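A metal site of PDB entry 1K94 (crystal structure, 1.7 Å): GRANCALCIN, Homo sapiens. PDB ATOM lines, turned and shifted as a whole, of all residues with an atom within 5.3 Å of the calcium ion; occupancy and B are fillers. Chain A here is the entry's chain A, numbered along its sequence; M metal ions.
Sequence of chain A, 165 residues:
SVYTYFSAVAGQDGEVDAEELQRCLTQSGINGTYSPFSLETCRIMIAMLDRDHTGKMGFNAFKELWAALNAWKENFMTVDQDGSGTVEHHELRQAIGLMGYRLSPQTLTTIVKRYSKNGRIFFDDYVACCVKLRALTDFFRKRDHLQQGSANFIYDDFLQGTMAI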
ATOM      1  N   ASP A  80       7.069  -6.963  10.814  1.00  0.00           N
ATOM      2  CA  ASP A  80       5.956  -6.650   9.917  1.00  0.00           C
ATOM      3  C   ASP A  80       5.887  -7.739   8.845  1.00  0.00           C
ATOM      4  O   ASP A  80       6.148  -7.497   7.673  1.00  0.00           O
ATOM      5  CB  ASP A  80       6.168  -5.291   9.250  1.00  0.00           C
ATOM      6  CG  ASP A  80       4.953  -4.822   8.479  1.00  0.00           C
ATOM      7  OD1 ASP A  80       5.084  -3.876   7.681  1.00  0.00           O
ATOM      8  OD2 ASP A  80       3.855  -5.391   8.683  1.00  0.00           O
ATOM      9  N   GLN A  81       5.515  -8.956   9.264  1.00  0.00           N
ATOM     10  CA  GLN A  81       5.441 -10.098   8.365  1.00  0.00           C
ATOM     11  C   GLN A  81       4.513  -9.976   7.159  1.00  0.00           C
ATOM     12  O   GLN A  81       4.776 -10.573   6.115  1.00  0.00           O
ATOM     13  CB  GLN A  81       5.062 -11.359   9.147  1.00  0.00           C
ATOM     14  CG  GLN A  81       6.014 -11.684  10.295  1.00  0.00           C
ATOM     15  CD  GLN A  81       5.476 -11.218  11.626  1.00  0.00           C
ATOM     16  OE1 GLN A  81       4.423 -10.591  11.704  1.00  0.00           O
ATOM     17  NE2 GLN A  81       6.194 -11.530  12.700  1.00  0.00           N
ATOM     18  N   ASP A  82       3.433  -9.203   7.285  1.00  0.00           N
ATOM     19  CA  ASP A  82       2.512  -9.048   6.165  1.00  0.00           C
ATOM     20  C   ASP A  82       2.807  -7.797   5.340  1.00  0.00           C
ATOM     21  O   ASP A  82       2.072  -7.461   4.412  1.00  0.00           O
ATOM     22  CB  ASP A  82       1.065  -9.050   6.661  1.00  0.00           C
ATOM     23  CG  ASP A  82       0.740  -7.900   7.610  1.00  0.00           C
ATOM     24  OD1 ASP A  82       1.653  -7.120   7.959  1.00  0.00           O
ATOM     25  OD2 ASP A  82      -0.445  -7.789   7.991  1.00  0.00           O
ATOM     26  N   GLY A  83       3.908  -7.128   5.679  1.00  0.00           N
ATOM     27  CA  GLY A  83       4.304  -5.921   4.957  1.00  0.00           C
ATOM     28  C   GLY A  83       3.219  -4.865   4.888  1.00  0.00           C
ATOM     29  O   GLY A  83       3.117  -4.154   3.881  1.00  0.00           O
ATOM     30  N   SER A  84       2.420  -4.753   5.938  1.00  0.00           N
ATOM     31  CA  SER A  84       1.339  -3.777   5.973  1.00  0.00           C
ATOM     32  C   SER A  84       1.841  -2.366   6.283  1.00  0.00           C
ATOM     33  O   SER A  84       1.095  -1.395   6.116  1.00  0.00           O
ATOM     34  CB  SER A  84       0.302  -4.185   7.013  1.00  0.00           C
ATOM     35  OG  SER A  84       0.853  -4.138   8.314  1.00  0.00           O
ATOM     36  N   GLY A  85       3.084  -2.263   6.726  1.00  0.00           N
ATOM     37  CA  GLY A  85       3.629  -0.963   7.071  1.00  0.00           C
ATOM     38  C   GLY A  85       3.076  -0.528   8.401  1.00  0.00           C
ATOM     39  O   GLY A  85       3.193   0.632   8.817  1.00  0.00           O
ATOM     40  N   THR A  86       2.440  -1.468   9.094  1.00  0.00           N
ATOM     41  CA  THR A  86       1.852  -1.209  10.404  1.00  0.00           C
ATOM     42  C   THR A  86       2.163  -2.416  11.274  1.00  0.00           C
ATOM     43  O   THR A  86       2.298  -3.522  10.774  1.00  0.00           O
ATOM     44  CB  THR A  86       0.323  -1.014  10.321  1.00  0.00           C
ATOM     45  OG1 THR A  86      -0.282  -2.196   9.768  1.00  0.00           O
ATOM     46  CG2 THR A  86      -0.038   0.172   9.449  1.00  0.00           C
ATOM     47  N   VAL A  87       2.279  -2.196  12.576  1.00  0.00           N
ATOM     48  CA  VAL A  87       2.568  -3.303  13.477  1.00  0.00           C
ATOM     49  C   VAL A  87       1.338  -3.669  14.306  1.00  0.00           C
ATOM     50  O   VAL A  87       0.835  -2.872  15.084  1.00  0.00           O
ATOM     51  CB  VAL A  87       3.772  -2.981  14.398  1.00  0.00           C
ATOM     52  CG1 VAL A  87       3.535  -1.709  15.177  1.00  0.00           C
ATOM     53  CG2 VAL A  87       4.020  -4.140  15.341  1.00  0.00           C
ATOM     54  N   GLU A  88       0.862  -4.897  14.110  1.00  0.00           N
ATOM     55  CA  GLU A  88      -0.296  -5.405  14.831  1.00  0.00           C
ATOM     56  C   GLU A  88       0.143  -6.055  16.142  1.00  0.00           C
ATOM     57  O   GLU A  88       1.327  -6.272  16.374  1.00  0.00           O
ATOM     58  CB  GLU A  88      -1.060  -6.418  13.974  1.00  0.00           C
ATOM     59  CG  GLU A  88      -1.878  -5.799  12.836  1.00  0.00           C
ATOM     60  CD  GLU A  88      -1.014  -5.064  11.826  1.00  0.00           C
ATOM     61  OE1 GLU A  88      -1.058  -3.809  11.805  1.00  0.00           O
ATOM     62  OE2 GLU A  88      -0.300  -5.739  11.056  1.00  0.00           O
ATOM     63  N   GLU A  91       2.762  -8.756  16.150  1.00  0.00           N
ATOM     64  CA  GLU A  91       4.012  -8.247  15.610  1.00  0.00           C
ATOM     65  C   GLU A  91       4.682  -7.347  16.657  1.00  0.00           C
ATOM     66  O   GLU A  91       5.894  -7.421  16.860  1.00  0.00           O
ATOM     67  CB  GLU A  91       3.744  -7.443  14.341  1.00  0.00           C
ATOM     68  CG  GLU A  91       2.939  -8.194  13.295  1.00  0.00           C
ATOM     69  CD  GLU A  91       2.723  -7.383  12.026  1.00  0.00           C
ATOM     70  OE1 GLU A  91       2.543  -6.154  12.141  1.00  0.00           O
ATOM     71  OE2 GLU A  91       2.726  -7.960  10.932  1.00  0.00           O
HETATM   72 CA    CA M   1       1.845  -5.720   9.889  1.00  0.00          CA
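The backbone NH of Gly 85 sits at hydrogen-bond distance from the side-chain carboxylate of Asp 80 (2.7 Å). The backbone NH of Gly 83 sits close to the side-chain carboxylate of Asp 80. OE1 of Gln 81 sits close to OE2 of Glu 91 (3.2 Å).
Within 4 Å of the calcium ion: Asp 80, Asp 82, Ser 84, Thr 86, Glu 88 and Glu 91.
The side-chain carboxylate (OD2) of Asp 80 binds the calcium ion, at 2.4 Å. OD1 of Asp 82 binds the calcium ion, at 2.4 Å. The calcium ion is bound by OE1 of Glu 91 (2.4 Å). The backbone carbonyl oxygen (O) of Thr 86 is bound to the calcium ion, at 2.4 Å. The side-chain carboxylate (OE2) of Glu 88 is bound to the calcium ion (2.4 Å). The calcium ion is bound by OG of Ser 84 (2.4 Å). The calcium ion is bound by OE2 of Glu 91 (2.6 Å). The calcium ion has seven donor atoms within binding distance.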
